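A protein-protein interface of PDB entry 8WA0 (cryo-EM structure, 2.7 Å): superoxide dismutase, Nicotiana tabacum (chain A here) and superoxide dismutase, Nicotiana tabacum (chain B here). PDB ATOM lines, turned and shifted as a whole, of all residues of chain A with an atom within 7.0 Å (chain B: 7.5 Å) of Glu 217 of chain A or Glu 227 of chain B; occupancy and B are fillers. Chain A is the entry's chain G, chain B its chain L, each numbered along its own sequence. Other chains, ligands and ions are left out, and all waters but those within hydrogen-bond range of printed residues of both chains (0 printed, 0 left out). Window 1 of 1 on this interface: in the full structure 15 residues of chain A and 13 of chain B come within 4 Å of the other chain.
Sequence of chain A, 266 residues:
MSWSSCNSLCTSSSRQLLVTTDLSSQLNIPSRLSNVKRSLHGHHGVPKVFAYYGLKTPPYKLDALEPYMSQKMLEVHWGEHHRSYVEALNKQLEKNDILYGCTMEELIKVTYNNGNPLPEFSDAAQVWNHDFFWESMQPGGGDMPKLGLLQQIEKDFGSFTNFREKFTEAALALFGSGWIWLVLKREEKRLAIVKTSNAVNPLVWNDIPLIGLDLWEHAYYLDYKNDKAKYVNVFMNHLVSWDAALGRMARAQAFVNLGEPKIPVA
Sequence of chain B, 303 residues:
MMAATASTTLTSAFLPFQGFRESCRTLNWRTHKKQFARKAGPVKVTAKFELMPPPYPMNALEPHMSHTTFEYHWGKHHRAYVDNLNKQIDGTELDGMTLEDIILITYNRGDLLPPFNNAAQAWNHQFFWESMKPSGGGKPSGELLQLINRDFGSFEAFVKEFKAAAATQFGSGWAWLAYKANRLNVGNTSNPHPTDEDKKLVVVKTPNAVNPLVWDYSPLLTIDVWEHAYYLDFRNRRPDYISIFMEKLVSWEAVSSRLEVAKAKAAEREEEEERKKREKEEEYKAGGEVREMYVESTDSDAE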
ATOM      1  N   MET A  73      30.879 -36.737   3.848  1.00  0.00           N
ATOM      2  CA  MET A  73      30.950 -35.313   3.580  1.00  0.00           C
ATOM      3  C   MET A  73      31.900 -34.661   4.562  1.00  0.00           C
ATOM      4  O   MET A  73      32.774 -33.890   4.171  1.00  0.00           O
ATOM      5  CB  MET A  73      29.557 -34.692   3.674  1.00  0.00           C
ATOM      6  CG  MET A  73      29.370 -33.472   2.793  1.00  0.00           C
ATOM      7  SD  MET A  73      27.637 -33.180   2.398  1.00  0.00           S
ATOM      8  CE  MET A  73      26.960 -32.908   4.031  1.00  0.00           C
ATOM      9  N   HIS A  81      40.032 -30.333   1.831  1.00  0.00           N
ATOM     10  CA  HIS A  81      40.067 -28.896   1.628  1.00  0.00           C
ATOM     11  C   HIS A  81      40.731 -28.185   2.789  1.00  0.00           C
ATOM     12  O   HIS A  81      41.607 -27.351   2.590  1.00  0.00           O
ATOM     13  CB  HIS A  81      38.655 -28.347   1.459  1.00  0.00           C
ATOM     14  CG  HIS A  81      37.767 -29.200   0.613  1.00  0.00           C
ATOM     15  ND1 HIS A  81      37.650 -29.029  -0.748  1.00  0.00           N
ATOM     16  CD2 HIS A  81      36.938 -30.219   0.937  1.00  0.00           C
ATOM     17  CE1 HIS A  81      36.794 -29.913  -1.229  1.00  0.00           C
ATOM     18  NE2 HIS A  81      36.348 -30.648  -0.226  1.00  0.00           N
ATOM     19  N   GLY A 176      26.880 -17.918  -5.764  1.00  0.00           N
ATOM     20  CA  GLY A 176      28.267 -18.249  -5.712  1.00  0.00           C
ATOM     21  C   GLY A 176      28.701 -18.816  -4.424  1.00  0.00           C
ATOM     22  O   GLY A 176      27.896 -19.329  -3.677  1.00  0.00           O
ATOM     23  N   SER A 177      30.010 -18.880  -4.214  1.00  0.00           N
ATOM     24  CA  SER A 177      30.546 -19.507  -3.011  1.00  0.00           C
ATOM     25  C   SER A 177      30.799 -18.470  -1.956  1.00  0.00           C
ATOM     26  O   SER A 177      31.556 -17.543  -2.184  1.00  0.00           O
ATOM     27  CB  SER A 177      31.840 -20.233  -3.336  1.00  0.00           C
ATOM     28  OG  SER A 177      31.624 -21.258  -4.284  1.00  0.00           O
ATOM     29  N   GLY A 178      30.172 -18.614  -0.797  1.00  0.00           N
ATOM     30  CA  GLY A 178      30.285 -17.599   0.230  1.00  0.00           C
ATOM     31  C   GLY A 178      29.876 -18.172   1.552  1.00  0.00           C
ATOM     32  O   GLY A 178      29.569 -19.350   1.629  1.00  0.00           O
ATOM     33  N   ASP A 214      28.751 -22.481   5.854  1.00  0.00           N
ATOM     34  CA  ASP A 214      29.481 -22.537   4.599  1.00  0.00           C
ATOM     35  C   ASP A 214      28.509 -22.783   3.464  1.00  0.00           C
ATOM     36  O   ASP A 214      27.870 -23.820   3.409  1.00  0.00           O
ATOM     37  CB  ASP A 214      30.509 -23.664   4.653  1.00  0.00           C
ATOM     38  CG  ASP A 214      31.566 -23.533   3.594  1.00  0.00           C
ATOM     39  OD1 ASP A 214      31.611 -22.473   2.949  1.00  0.00           O
ATOM     40  OD2 ASP A 214      32.358 -24.481   3.417  1.00  0.00           O
ATOM     41  N   LEU A 215      28.406 -21.837   2.548  1.00  0.00           N
ATOM     42  CA  LEU A 215      27.522 -21.995   1.407  1.00  0.00           C
ATOM     43  C   LEU A 215      28.330 -22.393   0.200  1.00  0.00           C
ATOM     44  O   LEU A 215      27.817 -22.403  -0.912  1.00  0.00           O
ATOM     45  CB  LEU A 215      26.727 -20.725   1.135  1.00  0.00           C
ATOM     46  CG  LEU A 215      25.784 -20.280   2.250  1.00  0.00           C
ATOM     47  CD1 LEU A 215      25.007 -19.050   1.814  1.00  0.00           C
ATOM     48  CD2 LEU A 215      24.836 -21.409   2.614  1.00  0.00           C
ATOM     49  N   TRP A 216      29.605 -22.692   0.402  1.00  0.00           N
ATOM     50  CA  TRP A 216      30.418 -23.183  -0.697  1.00  0.00           C
ATOM     51  C   TRP A 216      29.853 -24.524  -1.111  1.00  0.00           C
ATOM     52  O   TRP A 216      29.421 -25.301  -0.264  1.00  0.00           O
ATOM     53  CB  TRP A 216      31.874 -23.321  -0.278  1.00  0.00           C
ATOM     54  CG  TRP A 216      32.639 -22.033  -0.270  1.00  0.00           C
ATOM     55  CD1 TRP A 216      32.335 -20.903   0.424  1.00  0.00           C
ATOM     56  CD2 TRP A 216      33.852 -21.753  -0.978  1.00  0.00           C
ATOM     57  NE1 TRP A 216      33.272 -19.931   0.184  1.00  0.00           N
ATOM     58  CE2 TRP A 216      34.215 -20.428  -0.674  1.00  0.00           C
ATOM     59  CE3 TRP A 216      34.658 -22.490  -1.847  1.00  0.00           C
ATOM     60  CZ2 TRP A 216      35.351 -19.826  -1.206  1.00  0.00           C
ATOM     61  CZ3 TRP A 216      35.785 -21.891  -2.373  1.00  0.00           C
ATOM     62  CH2 TRP A 216      36.121 -20.572  -2.051  1.00  0.00           C
ATOM     63  N   GLU A 217      29.880 -24.834  -2.400  1.00  0.00           N
ATOM     64  CA  GLU A 217      29.245 -26.059  -2.883  1.00  0.00           C
ATOM     65  C   GLU A 217      29.814 -27.330  -2.308  1.00  0.00           C
ATOM     66  O   GLU A 217      29.068 -28.265  -2.043  1.00  0.00           O
ATOM     67  CB  GLU A 217      29.218 -26.106  -4.404  1.00  0.00           C
ATOM     68  CG  GLU A 217      28.236 -25.129  -5.017  1.00  0.00           C
ATOM     69  CD  GLU A 217      28.204 -25.211  -6.525  1.00  0.00           C
ATOM     70  OE1 GLU A 217      29.173 -25.727  -7.114  1.00  0.00           O
ATOM     71  OE2 GLU A 217      27.209 -24.754  -7.123  1.00  0.00           O
ATOM     72  N   HIS A 218      31.117 -27.371  -2.073  1.00  0.00           N
ATOM     73  CA  HIS A 218      31.722 -28.610  -1.612  1.00  0.00           C
ATOM     74  C   HIS A 218      31.072 -29.034  -0.323  1.00  0.00           C
ATOM     75  O   HIS A 218      30.919 -30.219  -0.062  1.00  0.00           O
ATOM     76  CB  HIS A 218      33.246 -28.504  -1.473  1.00  0.00           C
ATOM     77  CG  HIS A 218      33.714 -27.548  -0.422  1.00  0.00           C
ATOM     78  ND1 HIS A 218      33.898 -26.205  -0.666  1.00  0.00           N
ATOM     79  CD2 HIS A 218      34.082 -27.749   0.865  1.00  0.00           C
ATOM     80  CE1 HIS A 218      34.337 -25.615   0.431  1.00  0.00           C
ATOM     81  NE2 HIS A 218      34.454 -26.530   1.376  1.00  0.00           N
ATOM     82  N   ALA A 219      30.677 -28.070   0.482  1.00  0.00           N
ATOM     83  CA  ALA A 219      30.092 -28.382   1.771  1.00  0.00           C
ATOM     84  C   ALA A 219      28.802 -29.185   1.730  1.00  0.00           C
ATOM     85  O   ALA A 219      28.615 -30.064   2.557  1.00  0.00           O
ATOM     86  CB  ALA A 219      29.864 -27.096   2.549  1.00  0.00           C
ATOM     87  N   TYR A 220      27.891 -28.871   0.819  1.00  0.00           N
ATOM     88  CA  TYR A 220      26.601 -29.559   0.828  1.00  0.00           C
ATOM     89  C   TYR A 220      26.356 -30.511  -0.326  1.00  0.00           C
ATOM     90  O   TYR A 220      25.320 -31.167  -0.370  1.00  0.00           O
ATOM     91  CB  TYR A 220      25.467 -28.539   0.901  1.00  0.00           C
ATOM     92  CG  TYR A 220      25.338 -27.643  -0.308  1.00  0.00           C
ATOM     93  CD1 TYR A 220      26.102 -26.494  -0.429  1.00  0.00           C
ATOM     94  CD2 TYR A 220      24.431 -27.934  -1.318  1.00  0.00           C
ATOM     95  CE1 TYR A 220      25.982 -25.671  -1.527  1.00  0.00           C
ATOM     96  CE2 TYR A 220      24.307 -27.118  -2.421  1.00  0.00           C
ATOM     97  CZ  TYR A 220      25.085 -25.988  -2.520  1.00  0.00           C
ATOM     98  OH  TYR A 220      24.964 -25.166  -3.615  1.00  0.00           O
ATOM     99  N   TYR A 221      27.300 -30.623  -1.246  1.00  0.00           N
ATOM    100  CA  TYR A 221      27.070 -31.432  -2.445  1.00  0.00           C
ATOM    101  C   TYR A 221      26.932 -32.913  -2.239  1.00  0.00           C
ATOM    102  O   TYR A 221      25.948 -33.498  -2.657  1.00  0.00           O
ATOM    103  CB  TYR A 221      28.222 -31.227  -3.423  1.00  0.00           C
ATOM    104  CG  TYR A 221      27.830 -31.263  -4.874  1.00  0.00           C
ATOM    105  CD1 TYR A 221      27.239 -30.164  -5.476  1.00  0.00           C
ATOM    106  CD2 TYR A 221      28.074 -32.381  -5.651  1.00  0.00           C
ATOM    107  CE1 TYR A 221      26.881 -30.186  -6.807  1.00  0.00           C
ATOM    108  CE2 TYR A 221      27.725 -32.409  -6.984  1.00  0.00           C
ATOM    109  CZ  TYR A 221      27.125 -31.311  -7.556  1.00  0.00           C
ATOM    110  OH  TYR A 221      26.773 -31.339  -8.884  1.00  0.00           O
ATOM    111  N   LEU A 222      27.914 -33.530  -1.608  1.00  0.00           N
ATOM    112  CA  LEU A 222      27.910 -34.975  -1.499  1.00  0.00           C
ATOM    113  C   LEU A 222      26.521 -35.501  -1.196  1.00  0.00           C
ATOM    114  O   LEU A 222      26.018 -36.353  -1.921  1.00  0.00           O
ATOM    115  CB  LEU A 222      28.930 -35.463  -0.484  1.00  0.00           C
ATOM    116  CG  LEU A 222      30.340 -35.451  -1.066  1.00  0.00           C
ATOM    117  CD1 LEU A 222      31.367 -35.890  -0.040  1.00  0.00           C
ATOM    118  CD2 LEU A 222      30.388 -36.341  -2.296  1.00  0.00           C
ATOM    119  N   TYR A 224      23.425 -33.767  -0.917  1.00  0.00           N
ATOM    120  CA  TYR A 224      22.346 -33.187  -1.666  1.00  0.00           C
ATOM    121  C   TYR A 224      23.018 -32.376  -2.681  1.00  0.00           C
ATOM    122  O   TYR A 224      23.199 -31.191  -2.484  1.00  0.00           O
ATOM    123  CB  TYR A 224      21.546 -32.259  -0.798  1.00  0.00           C
ATOM    124  CG  TYR A 224      21.607 -32.581   0.677  1.00  0.00           C
ATOM    125  CD1 TYR A 224      20.968 -33.699   1.193  1.00  0.00           C
ATOM    126  CD2 TYR A 224      22.299 -31.763   1.556  1.00  0.00           C
ATOM    127  CE1 TYR A 224      21.030 -34.000   2.537  1.00  0.00           C
ATOM    128  CE2 TYR A 224      22.360 -32.057   2.904  1.00  0.00           C
ATOM    129  CZ  TYR A 224      21.720 -33.177   3.386  1.00  0.00           C
ATOM    130  OH  TYR A 224      21.772 -33.480   4.723  1.00  0.00           O
ATOM    131  N   LYS A 225      23.339 -32.963  -3.808  1.00  0.00           N
ATOM    132  CA  LYS A 225      24.109 -32.273  -4.800  1.00  0.00           C
ATOM    133  C   LYS A 225      23.417 -31.056  -5.233  1.00  0.00           C
ATOM    134  O   LYS A 225      24.032 -30.009  -5.333  1.00  0.00           O
ATOM    135  CB  LYS A 225      24.277 -33.155  -6.014  1.00  0.00           C
ATOM    136  CG  LYS A 225      24.852 -34.543  -5.743  1.00  0.00           C
ATOM    137  CD  LYS A 225      23.810 -35.582  -5.359  1.00  0.00           C
ATOM    138  CE  LYS A 225      24.448 -36.937  -5.111  1.00  0.00           C
ATOM    139  NZ  LYS A 225      23.433 -37.958  -4.730  1.00  0.00           N
ATOM    140  N   ASN A 226      22.134 -31.130  -5.482  1.00  0.00           N
ATOM    141  CA  ASN A 226      21.498 -29.895  -5.801  1.00  0.00           C
ATOM    142  C   ASN A 226      20.369 -29.484  -4.940  1.00  0.00           C
ATOM    143  O   ASN A 226      19.574 -28.653  -5.343  1.00  0.00           O
ATOM    144  CB  ASN A 226      21.238 -29.719  -7.281  1.00  0.00           C
ATOM    145  CG  ASN A 226      22.350 -28.958  -7.957  1.00  0.00           C
ATOM    146  OD1 ASN A 226      22.675 -29.193  -9.115  1.00  0.00           O
ATOM    147  ND2 ASN A 226      22.966 -28.057  -7.215  1.00  0.00           N
ATOM    148  N   THR B  69      26.331 -37.416 -13.539  1.00  0.00           N
ATOM    149  CA  THR B  69      26.834 -36.062 -13.401  1.00  0.00           C
ATOM    150  C   THR B  69      26.149 -35.202 -14.433  1.00  0.00           C
ATOM    151  O   THR B  69      25.718 -34.089 -14.143  1.00  0.00           O
ATOM    152  CB  THR B  69      28.350 -36.003 -13.641  1.00  0.00           C
ATOM    153  OG1 THR B  69      29.015 -36.878 -12.723  1.00  0.00           O
ATOM    154  CG2 THR B  69      28.875 -34.590 -13.448  1.00  0.00           C
ATOM    155  N   HIS B  73      23.993 -31.786 -13.956  1.00  0.00           N
ATOM    156  CA  HIS B  73      24.415 -30.527 -14.536  1.00  0.00           C
ATOM    157  C   HIS B  73      23.390 -29.944 -15.480  1.00  0.00           C
ATOM    158  O   HIS B  73      23.055 -28.770 -15.390  1.00  0.00           O
ATOM    159  CB  HIS B  73      25.724 -30.751 -15.291  1.00  0.00           C
ATOM    160  CG  HIS B  73      26.490 -29.498 -15.588  1.00  0.00           C
ATOM    161  ND1 HIS B  73      27.867 -29.465 -15.617  1.00  0.00           N
ATOM    162  CD2 HIS B  73      26.080 -28.238 -15.875  1.00  0.00           C
ATOM    163  CE1 HIS B  73      28.272 -28.243 -15.908  1.00  0.00           C
ATOM    164  NE2 HIS B  73      27.208 -27.479 -16.066  1.00  0.00           N
ATOM    165  N   HIS B  77      20.332 -28.006 -13.280  1.00  0.00           N
ATOM    166  CA  HIS B  77      20.675 -26.591 -13.316  1.00  0.00           C
ATOM    167  C   HIS B  77      19.939 -25.860 -14.395  1.00  0.00           C
ATOM    168  O   HIS B  77      19.371 -24.803 -14.160  1.00  0.00           O
ATOM    169  CB  HIS B  77      22.170 -26.406 -13.558  1.00  0.00           C
ATOM    170  CG  HIS B  77      23.021 -26.707 -12.365  1.00  0.00           C
ATOM    171  ND1 HIS B  77      23.471 -25.725 -11.507  1.00  0.00           N
ATOM    172  CD2 HIS B  77      23.514 -27.875 -11.892  1.00  0.00           C
ATOM    173  CE1 HIS B  77      24.197 -26.278 -10.553  1.00  0.00           C
ATOM    174  NE2 HIS B  77      24.239 -27.581 -10.764  1.00  0.00           N
ATOM    175  N   GLY B 171      36.994 -20.367  -6.609  1.00  0.00           N
ATOM    176  CA  GLY B 171      35.570 -20.332  -6.378  1.00  0.00           C
ATOM    177  C   GLY B 171      34.798 -20.549  -7.643  1.00  0.00           C
ATOM    178  O   GLY B 171      35.341 -21.010  -8.641  1.00  0.00           O
ATOM    179  N   SER B 172      33.521 -20.214  -7.607  1.00  0.00           N
ATOM    180  CA  SER B 172      32.677 -20.381  -8.772  1.00  0.00           C
ATOM    181  C   SER B 172      33.084 -19.491  -9.946  1.00  0.00           C
ATOM    182  O   SER B 172      33.407 -18.320  -9.755  1.00  0.00           O
ATOM    183  CB  SER B 172      31.242 -20.083  -8.358  1.00  0.00           C
ATOM    184  OG  SER B 172      31.133 -18.782  -7.813  1.00  0.00           O
ATOM    185  N   GLY B 173      33.063 -20.036 -11.161  1.00  0.00           N
ATOM    186  CA  GLY B 173      33.393 -19.239 -12.328  1.00  0.00           C
ATOM    187  C   GLY B 173      33.571 -19.948 -13.653  1.00  0.00           C
ATOM    188  O   GLY B 173      33.297 -21.139 -13.760  1.00  0.00           O
ATOM    189  N   ASP B 224      33.594 -24.973 -17.052  1.00  0.00           N
ATOM    190  CA  ASP B 224      32.870 -24.662 -15.843  1.00  0.00           C
ATOM    191  C   ASP B 224      33.770 -25.043 -14.678  1.00  0.00           C
ATOM    192  O   ASP B 224      34.096 -26.217 -14.517  1.00  0.00           O
ATOM    193  CB  ASP B 224      31.573 -25.458 -15.794  1.00  0.00           C
ATOM    194  CG  ASP B 224      30.501 -24.772 -14.995  1.00  0.00           C
ATOM    195  OD1 ASP B 224      30.749 -23.648 -14.530  1.00  0.00           O
ATOM    196  OD2 ASP B 224      29.406 -25.347 -14.848  1.00  0.00           O
ATOM    197  N   VAL B 225      34.174 -24.065 -13.862  1.00  0.00           N
ATOM    198  CA  VAL B 225      35.033 -24.332 -12.708  1.00  0.00           C
ATOM    199  C   VAL B 225      34.141 -24.436 -11.501  1.00  0.00           C
ATOM    200  O   VAL B 225      34.580 -24.869 -10.442  1.00  0.00           O
ATOM    201  CB  VAL B 225      36.052 -23.214 -12.509  1.00  0.00           C
ATOM    202  N   TRP B 226      32.894 -24.027 -11.649  1.00  0.00           N
ATOM    203  CA  TRP B 226      31.914 -24.139 -10.597  1.00  0.00           C
ATOM    204  C   TRP B 226      32.027 -25.577 -10.201  1.00  0.00           C
ATOM    205  O   TRP B 226      32.065 -26.461 -11.051  1.00  0.00           O
ATOM    206  CB  TRP B 226      30.513 -23.902 -11.129  1.00  0.00           C
ATOM    207  CG  TRP B 226      30.106 -22.488 -11.311  1.00  0.00           C
ATOM    208  CD1 TRP B 226      30.609 -21.600 -12.205  1.00  0.00           C
ATOM    209  CD2 TRP B 226      29.059 -21.808 -10.615  1.00  0.00           C
ATOM    210  NE1 TRP B 226      29.965 -20.392 -12.090  1.00  0.00           N
ATOM    211  CE2 TRP B 226      29.004 -20.496 -11.121  1.00  0.00           C
ATOM    212  CE3 TRP B 226      28.171 -22.178  -9.601  1.00  0.00           C
ATOM    213  CZ2 TRP B 226      28.097 -19.552 -10.650  1.00  0.00           C
ATOM    214  CZ3 TRP B 226      27.272 -21.238  -9.134  1.00  0.00           C
ATOM    215  CH2 TRP B 226      27.240 -19.941  -9.658  1.00  0.00           C
ATOM    216  N   GLU B 227      32.063 -25.828  -8.908  1.00  0.00           N
ATOM    217  CA  GLU B 227      32.265 -27.183  -8.438  1.00  0.00           C
ATOM    218  C   GLU B 227      31.240 -28.183  -8.932  1.00  0.00           C
ATOM    219  O   GLU B 227      31.579 -29.341  -9.149  1.00  0.00           O
ATOM    220  CB  GLU B 227      32.335 -27.202  -6.910  1.00  0.00           C
ATOM    221  CG  GLU B 227      33.627 -26.614  -6.359  1.00  0.00           C
ATOM    222  CD  GLU B 227      33.612 -26.439  -4.852  1.00  0.00           C
ATOM    223  OE1 GLU B 227      32.607 -25.927  -4.319  1.00  0.00           O
ATOM    224  OE2 GLU B 227      34.616 -26.797  -4.202  1.00  0.00           O
ATOM    225  N   HIS B 228      30.000 -27.759  -9.131  1.00  0.00           N
ATOM    226  CA  HIS B 228      28.986 -28.739  -9.499  1.00  0.00           C
ATOM    227  C   HIS B 228      29.400 -29.564 -10.690  1.00  0.00           C
ATOM    228  O   HIS B 228      29.089 -30.748 -10.760  1.00  0.00           O
ATOM    229  CB  HIS B 228      27.610 -28.090  -9.733  1.00  0.00           C
ATOM    230  CG  HIS B 228      27.527 -27.232 -10.957  1.00  0.00           C
ATOM    231  ND1 HIS B 228      27.777 -25.878 -10.934  1.00  0.00           N
ATOM    232  CD2 HIS B 228      27.186 -27.530 -12.232  1.00  0.00           C
ATOM    233  CE1 HIS B 228      27.610 -25.381 -12.147  1.00  0.00           C
ATOM    234  NE2 HIS B 228      27.253 -26.363 -12.954  1.00  0.00           N
ATOM    235  N   ALA B 229      30.121 -28.956 -11.618  1.00  0.00           N
ATOM    236  CA  ALA B 229      30.487 -29.655 -12.829  1.00  0.00           C
ATOM    237  C   ALA B 229      31.494 -30.774 -12.635  1.00  0.00           C
ATOM    238  O   ALA B 229      31.323 -31.846 -13.198  1.00  0.00           O
ATOM    239  CB  ALA B 229      31.017 -28.663 -13.842  1.00  0.00           C
ATOM    240  N   TYR B 230      32.537 -30.575 -11.846  1.00  0.00           N
ATOM    241  CA  TYR B 230      33.565 -31.613 -11.755  1.00  0.00           C
ATOM    242  C   TYR B 230      33.664 -32.323 -10.429  1.00  0.00           C
ATOM    243  O   TYR B 230      34.442 -33.265 -10.292  1.00  0.00           O
ATOM    244  CB  TYR B 230      34.931 -31.023 -12.086  1.00  0.00           C
ATOM    245  CG  TYR B 230      35.458 -30.041 -11.058  1.00  0.00           C
ATOM    246  CD1 TYR B 230      35.138 -28.691 -11.129  1.00  0.00           C
ATOM    247  CD2 TYR B 230      36.287 -30.461 -10.023  1.00  0.00           C
ATOM    248  CE1 TYR B 230      35.615 -27.794 -10.196  1.00  0.00           C
ATOM    249  CE2 TYR B 230      36.764 -29.570  -9.083  1.00  0.00           C
ATOM    250  CZ  TYR B 230      36.426 -28.240  -9.177  1.00  0.00           C
ATOM    251  OH  TYR B 230      36.906 -27.350  -8.247  1.00  0.00           O
ATOM    252  N   TYR B 231      32.885 -31.900  -9.450  1.00  0.00           N
ATOM    253  CA  TYR B 231      33.029 -32.469  -8.115  1.00  0.00           C
ATOM    254  C   TYR B 231      32.743 -33.953  -8.050  1.00  0.00           C
ATOM    255  O   TYR B 231      33.419 -34.687  -7.336  1.00  0.00           O
ATOM    256  CB  TYR B 231      32.134 -31.723  -7.132  1.00  0.00           C
ATOM    257  CG  TYR B 231      32.469 -31.968  -5.684  1.00  0.00           C
ATOM    258  CD1 TYR B 231      33.656 -31.499  -5.143  1.00  0.00           C
ATOM    259  CD2 TYR B 231      31.597 -32.657  -4.857  1.00  0.00           C
ATOM    260  CE1 TYR B 231      33.968 -31.717  -3.817  1.00  0.00           C
ATOM    261  CE2 TYR B 231      31.900 -32.879  -3.529  1.00  0.00           C
ATOM    262  CZ  TYR B 231      33.087 -32.407  -3.015  1.00  0.00           C
ATOM    263  OH  TYR B 231      33.395 -32.625  -1.694  1.00  0.00           O
ATOM    264  N   LEU B 232      31.727 -34.396  -8.768  1.00  0.00           N
ATOM    265  CA  LEU B 232      31.337 -35.796  -8.676  1.00  0.00           C
ATOM    266  C   LEU B 232      32.427 -36.758  -9.109  1.00  0.00           C
ATOM    267  O   LEU B 232      32.812 -37.641  -8.345  1.00  0.00           O
ATOM    268  CB  LEU B 232      30.050 -36.032  -9.459  1.00  0.00           C
ATOM    269  CG  LEU B 232      28.823 -35.441  -8.770  1.00  0.00           C
ATOM    270  CD1 LEU B 232      27.629 -35.346  -9.702  1.00  0.00           C
ATOM    271  CD2 LEU B 232      28.475 -36.231  -7.519  1.00  0.00           C
ATOM    272  N   ASP B 233      32.930 -36.596 -10.322  1.00  0.00           N
ATOM    273  CA  ASP B 233      33.918 -37.535 -10.829  1.00  0.00           C
ATOM    274  C   ASP B 233      35.193 -37.530 -10.013  1.00  0.00           C
ATOM    275  O   ASP B 233      35.720 -38.585  -9.674  1.00  0.00           O
ATOM    276  CB  ASP B 233      34.252 -37.174 -12.270  1.00  0.00           C
ATOM    277  CG  ASP B 233      33.012 -36.978 -13.124  1.00  0.00           C
ATOM    278  OD1 ASP B 233      31.942 -37.512 -12.762  1.00  0.00           O
ATOM    279  OD2 ASP B 233      33.106 -36.292 -14.165  1.00  0.00           O
ATOM    280  N   PHE B 234      35.692 -36.346  -9.688  1.00  0.00           N
ATOM    281  CA  PHE B 234      36.881 -36.249  -8.859  1.00  0.00           C
ATOM    282  C   PHE B 234      36.543 -35.290  -7.748  1.00  0.00           C
ATOM    283  O   PHE B 234      36.111 -34.174  -8.016  1.00  0.00           O
ATOM    284  CB  PHE B 234      38.052 -35.722  -9.679  1.00  0.00           C
ATOM    285  N   ASN B 236      37.220 -32.584  -5.789  1.00  0.00           N
ATOM    286  CA  ASN B 236      38.154 -31.473  -5.628  1.00  0.00           C
ATOM    287  C   ASN B 236      39.494 -31.654  -6.306  1.00  0.00           C
ATOM    288  O   ASN B 236      40.430 -30.914  -6.025  1.00  0.00           O
ATOM    289  CB  ASN B 236      38.344 -31.071  -4.169  1.00  0.00           C
ATOM    290  CG  ASN B 236      38.519 -29.573  -4.008  1.00  0.00           C
ATOM    291  OD1 ASN B 236      39.360 -29.108  -3.239  1.00  0.00           O
ATOM    292  ND2 ASN B 236      37.734 -28.807  -4.755  1.00  0.00           N
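Of the 17 printed residues of chain A, 8 touch a printed residue of chain B. Printed residues of chain A that touch a printed residue of chain B: His 81, Gly 176, Ser 177, Glu 217, His 218, Tyr 221, Leu 222 and Asn 226. Hydrophobic or aromatic side chains of chain A that line the printed part of chain B: His 81, His 218, Tyr 221 and Leu 222. Along chain A the printed residues that touch a printed residue of chain B span positions 81 to 226. Among the printed residues, no Asp or Glu carboxylate lies within 4 Å of a Lys or Arg side-chain nitrogen of the other chain.
Glu 227 of chain B touches just these residues of chain A: Glu 217 and His 218. Of the printed residues of chain B, Gly 176 of chain A touches Ser 172. Printed residues of chain B within 4 Å of Tyr 221 of chain A: His 228, Tyr 231 and Leu 232. Lys 225 of chain A touches none of the printed residues of chain B. Val 225 of chain B touches none of the printed residues of chain A. The nearest printed residue of chain A that does not touch His 228 of chain B is Asn 226 of chain A (5.1 Å).
The backbone NH (N) of His 228 of chain B sits at hydrogen-bond distance from the side-chain carboxylate (OE1) of Glu 217 of chain A, at 3.0 Å. OD1 of Asn 226 of chain A is in hydrogen-bond range of NE2 of His 77 of chain B (2.8 Å). The side-chain amide oxygen of Asn 236 of chain B lies within hydrogen-bond range of a ring nitrogen (ND1) of His 81 of chain A (3.0 Å). The side-chain carboxylate (OE1) of Glu 227 of chain B sits at hydrogen-bond distance from the backbone NH (N) of His 218 of chain A, 3.1 Å away. O of His 228 of chain B sits at hydrogen-bond distance from OH of Tyr 221 of chain A, 3.0 Å away. The backbone NH of Glu 227 of chain B sits at hydrogen-bond distance from the side-chain carboxylate of Glu 217 of chain A, at 3.4 Å.
Tyr 231 of chain B touches His 81 of chain A (OH to NE2, 3.8 Å). CA of Gly 176 of chain A touches OG of Ser 172 of chain B (3.6 Å). OG of Ser 172 of chain B touches N of Ser 177 of chain A (3.8 Å). OE2 of Glu 217 of chain A touches CE3 of Trp 226 of chain B (3.7 Å). OH of Tyr 231 of chain B touches O of His 218 of chain A (3.8 Å). Tyr 231 of chain B touches Tyr 221 of chain A (CD2 to CD2, 3.6 Å). CE2 of Tyr 221 of chain A touches CG of Leu 232 of chain B (3.7 Å). Leu 222 of chain A touches Tyr 231 of chain B.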
